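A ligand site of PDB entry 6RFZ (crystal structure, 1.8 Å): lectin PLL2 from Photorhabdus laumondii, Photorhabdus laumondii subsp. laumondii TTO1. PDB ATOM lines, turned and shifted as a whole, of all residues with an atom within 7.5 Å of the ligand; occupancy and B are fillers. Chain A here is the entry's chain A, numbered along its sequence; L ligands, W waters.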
ATOM      1  N   ASN A  89       1.792   2.740 -28.619  1.00  0.00           N
ATOM      2  CA  ASN A  89       0.837   3.015 -29.730  1.00  0.00           C
ATOM      3  C   ASN A  89       0.882   4.520 -30.023  1.00  0.00           C
ATOM      4  O   ASN A  89       1.289   5.285 -29.126  1.00  0.00           O
ATOM      5  CB  ASN A  89      -0.575   2.529 -29.393  1.00  0.00           C
ATOM      6  CG  ASN A  89      -0.735   1.035 -29.542  1.00  0.00           C
ATOM      7  OD1 ASN A  89      -0.817   0.536 -30.663  1.00  0.00           O
ATOM      8  ND2 ASN A  89      -0.821   0.313 -28.433  1.00  0.00           N
ATOM      9  N   ASP A  91      -1.342   6.579 -30.043  1.00  0.00           N
ATOM     10  CA  ASP A  91      -2.313   7.278 -29.148  1.00  0.00           C
ATOM     11  C   ASP A  91      -1.782   7.269 -27.701  1.00  0.00           C
ATOM     12  O   ASP A  91      -2.536   7.678 -26.801  1.00  0.00           O
ATOM     13  CB  ASP A  91      -3.703   6.640 -29.238  1.00  0.00           C
ATOM     14  CG  ASP A  91      -3.782   5.192 -28.759  1.00  0.00           C
ATOM     15  OD1 ASP A  91      -2.737   4.626 -28.383  1.00  0.00           O
ATOM     16  OD2 ASP A  91      -4.900   4.653 -28.745  1.00  0.00           O
ATOM     17  N   ARG A  93      -0.978   4.731 -25.714  1.00  0.00           N
ATOM     18  CA  ARG A  93      -1.281   3.493 -24.934  1.00  0.00           C
ATOM     19  C   ARG A  93      -0.116   2.510 -25.086  1.00  0.00           C
ATOM     20  O   ARG A  93       0.214   2.160 -26.240  1.00  0.00           O
ATOM     21  CB  ARG A  93      -2.592   2.863 -25.397  1.00  0.00           C
ATOM     22  CG  ARG A  93      -3.832   3.670 -25.035  1.00  0.00           C
ATOM     23  CD  ARG A  93      -5.128   3.026 -25.529  1.00  0.00           C
ATOM     24  NE  ARG A  93      -5.028   2.628 -26.936  1.00  0.00           N
ATOM     25  CZ  ARG A  93      -4.686   1.423 -27.377  1.00  0.00           C
ATOM     26  NH1 ARG A  93      -4.395   0.439 -26.534  1.00  0.00           N
ATOM     27  NH2 ARG A  93      -4.620   1.211 -28.673  1.00  0.00           N
ATOM     28  N   LEU A  94       0.511   2.112 -23.974  1.00  0.00           N
ATOM     29  CA  LEU A  94       1.598   1.103 -23.965  1.00  0.00           C
ATOM     30  C   LEU A  94       1.004  -0.258 -24.316  1.00  0.00           C
ATOM     31  O   LEU A  94      -0.145  -0.534 -23.916  1.00  0.00           O
ATOM     32  CB  LEU A  94       2.285   1.047 -22.594  1.00  0.00           C
ATOM     33  CG  LEU A  94       3.048   2.297 -22.161  1.00  0.00           C
ATOM     34  CD1 LEU A  94       3.889   2.010 -20.925  1.00  0.00           C
ATOM     35  CD2 LEU A  94       3.937   2.818 -23.290  1.00  0.00           C
ATOM     36  N   GLU A  95       1.755  -1.077 -25.054  1.00  0.00           N
ATOM     37  CA  GLU A  95       1.365  -2.458 -25.416  1.00  0.00           C
ATOM     38  C   GLU A  95       2.596  -3.362 -25.294  1.00  0.00           C
ATOM     39  O   GLU A  95       3.653  -2.997 -25.873  1.00  0.00           O
ATOM     40  CB  GLU A  95       0.770  -2.475 -26.822  1.00  0.00           C
ATOM     41  CG  GLU A  95       0.017  -3.755 -27.144  1.00  0.00           C
ATOM     42  CD  GLU A  95      -1.049  -3.604 -28.220  1.00  0.00           C
ATOM     43  OE1 GLU A  95      -1.442  -2.448 -28.530  1.00  0.00           O
ATOM     44  OE2 GLU A  95      -1.495  -4.643 -28.736  1.00  0.00           O
ATOM     45  N   PHE A  97       4.376  -7.166 -25.762  1.00  0.00           N
ATOM     46  CA  PHE A  97       4.379  -8.411 -26.562  1.00  0.00           C
ATOM     47  C   PHE A  97       5.389  -9.385 -25.958  1.00  0.00           C
ATOM     48  O   PHE A  97       6.499  -8.951 -25.604  1.00  0.00           O
ATOM     49  CB  PHE A  97       4.688  -8.071 -28.024  1.00  0.00           C
ATOM     50  CG  PHE A  97       3.723  -7.094 -28.640  1.00  0.00           C
ATOM     51  CD1 PHE A  97       3.927  -5.725 -28.508  1.00  0.00           C
ATOM     52  CD2 PHE A  97       2.611  -7.534 -29.329  1.00  0.00           C
ATOM     53  CE1 PHE A  97       3.034  -4.823 -29.066  1.00  0.00           C
ATOM     54  CE2 PHE A  97       1.717  -6.631 -29.887  1.00  0.00           C
ATOM     55  CZ  PHE A  97       1.931  -5.280 -29.756  1.00  0.00           C
ATOM     56  N   HIS A 107      -0.174 -10.625 -26.024  1.00  0.00           N
ATOM     57  CA  HIS A 107      -0.052  -9.167 -25.824  1.00  0.00           C
ATOM     58  C   HIS A 107      -1.084  -8.704 -24.811  1.00  0.00           C
ATOM     59  O   HIS A 107      -2.051  -9.438 -24.531  1.00  0.00           O
ATOM     60  CB  HIS A 107      -0.092  -8.420 -27.169  1.00  0.00           C
ATOM     61  CG  HIS A 107      -1.438  -8.350 -27.805  1.00  0.00           C
ATOM     62  ND1 HIS A 107      -1.942  -7.162 -28.297  1.00  0.00           N
ATOM     63  CD2 HIS A 107      -2.383  -9.293 -28.026  1.00  0.00           C
ATOM     64  CE1 HIS A 107      -3.143  -7.380 -28.801  1.00  0.00           C
ATOM     65  NE2 HIS A 107      -3.432  -8.677 -28.642  1.00  0.00           N
ATOM     66  N   ILE A 108      -0.820  -7.529 -24.237  1.00  0.00           N
ATOM     67  CA  ILE A 108      -1.635  -6.834 -23.211  1.00  0.00           C
ATOM     68  C   ILE A 108      -1.397  -5.346 -23.441  1.00  0.00           C
ATOM     69  O   ILE A 108      -0.269  -4.989 -23.838  1.00  0.00           O
ATOM     70  CB  ILE A 108      -1.232  -7.323 -21.798  1.00  0.00           C
ATOM     71  CG1 ILE A 108      -2.170  -6.795 -20.721  1.00  0.00           C
ATOM     72  CG2 ILE A 108       0.224  -6.987 -21.504  1.00  0.00           C
ATOM     73  CD1 ILE A 108      -2.016  -7.498 -19.388  1.00  0.00           C
ATOM     74  N   TRP A 109      -2.407  -4.516 -23.249  1.00  0.00           N
ATOM     75  CA  TRP A 109      -2.363  -3.079 -23.622  1.00  0.00           C
ATOM     76  C   TRP A 109      -3.032  -2.242 -22.540  1.00  0.00           C
ATOM     77  O   TRP A 109      -3.935  -2.763 -21.855  1.00  0.00           O
ATOM     78  CB  TRP A 109      -3.010  -2.861 -24.993  1.00  0.00           C
ATOM     79  CG  TRP A 109      -4.430  -3.344 -25.073  1.00  0.00           C
ATOM     80  CD1 TRP A 109      -5.554  -2.617 -24.818  1.00  0.00           C
ATOM     81  CD2 TRP A 109      -4.877  -4.665 -25.399  1.00  0.00           C
ATOM     82  NE1 TRP A 109      -6.664  -3.391 -24.975  1.00  0.00           N
ATOM     83  CE2 TRP A 109      -6.283  -4.656 -25.323  1.00  0.00           C
ATOM     84  CE3 TRP A 109      -4.229  -5.855 -25.735  1.00  0.00           C
ATOM     85  CZ2 TRP A 109      -7.054  -5.786 -25.586  1.00  0.00           C
ATOM     86  CZ3 TRP A 109      -4.988  -6.978 -26.002  1.00  0.00           C
ATOM     87  CH2 TRP A 109      -6.385  -6.940 -25.924  1.00  0.00           C
ATOM     88  N   GLN A 110      -2.585  -0.998 -22.387  1.00  0.00           N
ATOM     89  CA  GLN A 110      -3.299   0.027 -21.604  1.00  0.00           C
ATOM     90  C   GLN A 110      -4.614   0.327 -22.328  1.00  0.00           C
ATOM     91  O   GLN A 110      -4.589   0.414 -23.577  1.00  0.00           O
ATOM     92  CB  GLN A 110      -2.417   1.259 -21.418  1.00  0.00           C
ATOM     93  CG  GLN A 110      -1.286   1.031 -20.415  1.00  0.00           C
ATOM     94  CD  GLN A 110      -0.357   2.210 -20.315  1.00  0.00           C
ATOM     95  OE1 GLN A 110      -0.205   3.003 -21.244  1.00  0.00           O
ATOM     96  NE2 GLN A 110       0.290   2.333 -19.163  1.00  0.00           N
ATOM     97  N   THR A 111      -5.716   0.443 -21.592  1.00  0.00           N
ATOM     98  CA  THR A 111      -7.062   0.744 -22.146  1.00  0.00           C
ATOM     99  C   THR A 111      -7.190   2.261 -22.347  1.00  0.00           C
ATOM    100  O   THR A 111      -8.018   2.663 -23.175  1.00  0.00           O
ATOM    101  CB  THR A 111      -8.162   0.173 -21.238  1.00  0.00           C
ATOM    102  OG1 THR A 111      -7.957   0.671 -19.919  1.00  0.00           O
ATOM    103  CG2 THR A 111      -8.171  -1.339 -21.238  1.00  0.00           C
ATOM    104  N   SER A 118      -5.518  -4.006 -20.024  1.00  0.00           N
ATOM    105  CA  SER A 118      -6.399  -5.116 -20.460  1.00  0.00           C
ATOM    106  C   SER A 118      -5.961  -6.416 -19.769  1.00  0.00           C
ATOM    107  O   SER A 118      -4.999  -6.368 -18.971  1.00  0.00           O
ATOM    108  CB  SER A 118      -6.357  -5.292 -21.953  1.00  0.00           C
ATOM    109  OG  SER A 118      -5.120  -5.868 -22.350  1.00  0.00           O
ATOM    110  N   GLN A 121      -4.087 -11.311 -24.153  1.00  0.00           N
ATOM    111  CA  GLN A 121      -4.811 -11.943 -25.289  1.00  0.00           C
ATOM    112  C   GLN A 121      -3.773 -12.614 -26.190  1.00  0.00           C
ATOM    113  O   GLN A 121      -2.658 -12.051 -26.324  1.00  0.00           O
ATOM    114  CB  GLN A 121      -5.652 -10.890 -26.019  1.00  0.00           C
ATOM    115  CG  GLN A 121      -6.054 -11.282 -27.433  1.00  0.00           C
ATOM    116  CD  GLN A 121      -6.715 -10.146 -28.166  1.00  0.00           C
ATOM    117  OE1 GLN A 121      -6.142  -9.559 -29.093  1.00  0.00           O
ATOM    118  NE2 GLN A 121      -7.925  -9.798 -27.733  1.00  0.00           N
ATOM    119  N   LEU A 123      -2.271 -13.790 -29.836  1.00  0.00           N
ATOM    120  CA  LEU A 123      -2.225 -13.524 -31.297  1.00  0.00           C
ATOM    121  C   LEU A 123      -1.819 -14.801 -32.017  1.00  0.00           C
ATOM    122  O   LEU A 123      -1.556 -14.726 -33.236  1.00  0.00           O
ATOM    123  CB  LEU A 123      -1.224 -12.387 -31.554  1.00  0.00           C
ATOM    124  CG  LEU A 123      -1.680 -11.019 -31.061  1.00  0.00           C
ATOM    125  CD1 LEU A 123      -0.565  -9.992 -31.215  1.00  0.00           C
ATOM    126  CD2 LEU A 123      -2.928 -10.564 -31.798  1.00  0.00           C
ATOM    127  N   ILE A 141       0.872  -1.164 -35.596  1.00  0.00           N
ATOM    128  CA  ILE A 141       2.002  -1.918 -34.983  1.00  0.00           C
ATOM    129  C   ILE A 141       2.255  -3.178 -35.828  1.00  0.00           C
ATOM    130  O   ILE A 141       1.286  -3.841 -36.217  1.00  0.00           O
ATOM    131  CB  ILE A 141       1.755  -2.268 -33.506  1.00  0.00           C
ATOM    132  CG1 ILE A 141       1.780  -1.007 -32.642  1.00  0.00           C
ATOM    133  CG2 ILE A 141       2.765  -3.309 -33.025  1.00  0.00           C
ATOM    134  CD1 ILE A 141       1.638  -1.261 -31.166  1.00  0.00           C
ATOM    135  N   GLN A 157      -1.433  -4.986 -36.546  1.00  0.00           N
ATOM    136  CA  GLN A 157      -2.731  -4.278 -36.414  1.00  0.00           C
ATOM    137  C   GLN A 157      -3.240  -3.955 -37.825  1.00  0.00           C
ATOM    138  O   GLN A 157      -2.397  -3.571 -38.662  1.00  0.00           O
ATOM    139  CB  GLN A 157      -2.554  -2.997 -35.597  1.00  0.00           C
ATOM    140  CG  GLN A 157      -2.299  -3.239 -34.112  1.00  0.00           C
ATOM    141  CD  GLN A 157      -1.941  -1.966 -33.383  1.00  0.00           C
ATOM    142  OE1 GLN A 157      -1.456  -0.986 -33.969  1.00  0.00           O
ATOM    143  NE2 GLN A 157      -2.155  -1.957 -32.069  1.00  0.00           N
ATOM    144  N   ALA A 159      -5.771  -1.741 -38.302  1.00  0.00           N
ATOM    145  CA  ALA A 159      -6.146  -0.307 -38.152  1.00  0.00           C
ATOM    146  C   ALA A 159      -5.223   0.351 -37.120  1.00  0.00           C
ATOM    147  O   ALA A 159      -4.660  -0.379 -36.288  1.00  0.00           O
ATOM    148  CB  ALA A 159      -7.600  -0.193 -37.769  1.00  0.00           C
ATOM    149  N   ALA A 160      -5.065   1.674 -37.184  1.00  0.00           N
ATOM    150  CA  ALA A 160      -4.161   2.452 -36.309  1.00  0.00           C
ATOM    151  C   ALA A 160      -4.455   2.087 -34.848  1.00  0.00           C
ATOM    152  O   ALA A 160      -5.618   2.231 -34.430  1.00  0.00           O
ATOM    153  CB  ALA A 160      -4.315   3.931 -36.557  1.00  0.00           C
ATOM    154  N   HIS A 161      -3.428   1.630 -34.114  1.00  0.00           N
ATOM    155  CA  HIS A 161      -3.478   1.291 -32.665  1.00  0.00           C
ATOM    156  C   HIS A 161      -4.776   0.524 -32.336  1.00  0.00           C
ATOM    157  O   HIS A 161      -5.423   0.843 -31.320  1.00  0.00           O
ATOM    158  CB  HIS A 161      -3.312   2.553 -31.813  1.00  0.00           C
ATOM    159  CG  HIS A 161      -4.226   3.683 -32.175  1.00  0.00           C
ATOM    160  ND1 HIS A 161      -5.548   3.723 -31.786  1.00  0.00           N
ATOM    161  CD2 HIS A 161      -4.007   4.811 -32.890  1.00  0.00           C
ATOM    162  CE1 HIS A 161      -6.113   4.816 -32.244  1.00  0.00           C
ATOM    163  NE2 HIS A 161      -5.179   5.505 -32.921  1.00  0.00           N
ATOM    164  N   SER A 162      -5.129  -0.465 -33.160  1.00  0.00           N
ATOM    165  CA  SER A 162      -6.442  -1.166 -33.070  1.00  0.00           C
ATOM    166  C   SER A 162      -6.373  -2.562 -33.677  1.00  0.00           C
ATOM    167  O   SER A 162      -5.575  -2.782 -34.625  1.00  0.00           O
ATOM    168  CB  SER A 162      -7.527  -0.351 -33.724  1.00  0.00           C
ATOM    169  OG  SER A 162      -8.787  -0.987 -33.589  1.00  0.00           O
ATOM    170  N   GLY A 163      -7.202  -3.476 -33.167  1.00  0.00           N
ATOM    171  CA  GLY A 163      -7.535  -4.758 -33.806  1.00  0.00           C
ATOM    172  C   GLY A 163      -8.572  -4.566 -34.901  1.00  0.00           C
ATOM    173  O   GLY A 163      -9.046  -3.448 -35.135  1.00  0.00           O
ATOM    174  N   PRO A 164      -8.965  -5.639 -35.631  1.00  0.00           N
ATOM    175  CA  PRO A 164      -8.372  -6.965 -35.437  1.00  0.00           C
ATOM    176  C   PRO A 164      -6.935  -6.981 -35.983  1.00  0.00           C
ATOM    177  O   PRO A 164      -6.568  -6.078 -36.707  1.00  0.00           O
ATOM    178  CB  PRO A 164      -9.292  -7.881 -36.247  1.00  0.00           C
ATOM    179  CG  PRO A 164      -9.797  -6.983 -37.356  1.00  0.00           C
ATOM    180  CD  PRO A 164      -9.967  -5.624 -36.705  1.00  0.00           C
ATOM    181  N   TRP A 165      -6.156  -8.005 -35.608  1.00  0.00           N
ATOM    182  CA  TRP A 165      -4.778  -8.207 -36.123  1.00  0.00           C
ATOM    183  C   TRP A 165      -4.849  -9.009 -37.422  1.00  0.00           C
ATOM    184  O   TRP A 165      -5.849  -9.718 -37.622  1.00  0.00           O
ATOM    185  CB  TRP A 165      -3.889  -8.878 -35.071  1.00  0.00           C
ATOM    186  CG  TRP A 165      -3.438  -7.930 -34.017  1.00  0.00           C
ATOM    187  CD1 TRP A 165      -4.208  -7.323 -33.065  1.00  0.00           C
ATOM    188  CD2 TRP A 165      -2.103  -7.430 -33.823  1.00  0.00           C
ATOM    189  NE1 TRP A 165      -3.441  -6.496 -32.286  1.00  0.00           N
ATOM    190  CE2 TRP A 165      -2.143  -6.549 -32.726  1.00  0.00           C
ATOM    191  CE3 TRP A 165      -0.873  -7.658 -34.452  1.00  0.00           C
ATOM    192  CZ2 TRP A 165      -1.009  -5.894 -32.260  1.00  0.00           C
ATOM    193  CZ3 TRP A 165       0.250  -7.010 -33.982  1.00  0.00           C
ATOM    194  CH2 TRP A 165       0.187  -6.143 -32.900  1.00  0.00           C
HETATM  195  C1  LIG L   1      -5.814  -4.769 -30.041  1.00  0.00           C
HETATM  196  C2  LIG L   1      -4.644  -3.979 -29.483  1.00  0.00           C
HETATM  197  C3  LIG L   1      -5.103  -2.523 -29.366  1.00  0.00           C
HETATM  198  C4  LIG L   1      -6.347  -2.448 -28.480  1.00  0.00           C
HETATM  199  C5  LIG L   1      -6.944  -1.060 -28.417  1.00  0.00           C
HETATM  200  C6  LIG L   1      -7.014  -4.657 -29.112  1.00  0.00           C
HETATM  201  O1  LIG L   1      -8.118  -5.373 -29.673  1.00  0.00           O
HETATM  202  O2  LIG L   1      -5.491  -6.141 -30.186  1.00  0.00           O
HETATM  203  O3  LIG L   1      -3.502  -4.115 -30.344  1.00  0.00           O
HETATM  204  O4  LIG L   1      -4.076  -1.701 -28.821  1.00  0.00           O
HETATM  205  O5  LIG L   1      -7.381  -3.298 -28.969  1.00  0.00           O
HETATM  206  O6  LIG L   1      -8.210  -1.143 -27.762  1.00  0.00           O
HETATM  207  O   HOH W   1      -9.271  -2.747 -31.203  1.00  0.00           O
HETATM  208  O   HOH W   2      -8.146   0.615 -25.809  1.00  0.00           O
HETATM  209  O   HOH W   3     -10.911   0.469 -28.628  1.00  0.00           O
HETATM  210  O   HOH W   4     -10.213  -5.855 -27.582  1.00  0.00           O
HETATM  211  O   HOH W   5      -7.162  -7.858 -30.908  1.00  0.00           O
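An oxygen (O3) of the ligand sits at hydrogen-bond distance from the side-chain carboxylate (OE2) of Glu 95.
The guanidinium group (NH2) of Arg 93 sits at hydrogen-bond distance from an oxygen (O4) of the ligand.
O2 of the ligand sits at hydrogen-bond distance from NE1 of Trp 165 (3.0 Å).
An oxygen (O3) of the ligand is in hydrogen-bond range of the side-chain amide nitrogen of Gln 157 (3.1 Å).
Water W5 lies within hydrogen-bond range of O2 of the ligand (2.5 Å) and OE1 of Gln 121 (2.7 Å).
Water W2 bridges an oxygen (O6) of the ligand (2.6 Å) and the backbone carbonyl oxygen of Thr 111 (3.3 Å).
Water W1 lies within hydrogen-bond range of the backbone NH (N) of Gly 163 (2.9 Å), an oxygen (O5) of the ligand (3.0 Å) and the side-chain hydroxyl (OG) of Ser 162 (3.0 Å).
The side-chain amide nitrogen (ND2) of Asn 89 sits at hydrogen-bond distance from the backbone carbonyl oxygen (O) of Arg 93.
O of Gln 110 is in hydrogen-bond range of NH1 of Arg 93 (3.0 Å).
The guanidinium group of Arg 93 sits at hydrogen-bond distance from the backbone carbonyl oxygen of His 161 (2.8 Å).
The backbone NH of Ile 141 sits at hydrogen-bond distance from the side-chain amide oxygen of Gln 157, at 2.8 Å.
OE1 of Glu 95 is in hydrogen-bond range of ND2 of Asn 89, at 2.8 Å.
The backbone NH (N) of His 161 is in hydrogen-bond range of the side-chain amide oxygen (OE1) of Gln 157, at 3.3 Å.
NE of Arg 93 lies within salt-bridge range of OD2 of Asp 91, 2.7 Å away.
The backbone carbonyl oxygen of Trp 109 is in hydrogen-bond range of the backbone NH of Ser 118, at 2.7 Å.
Merely in contact with the ligand: His 107, Trp 109, Gln 121, Gly 163, His 161 and Asn 89.
Within 4 Å of the ligand: Asn 89, Arg 93, Glu 95, His 107, Trp 109, Gln 121, Gln 157, His 161, Gly 163 and Trp 165.
The nearest printed residue that does not touch the ligand is Ser 162 (4.2 Å).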
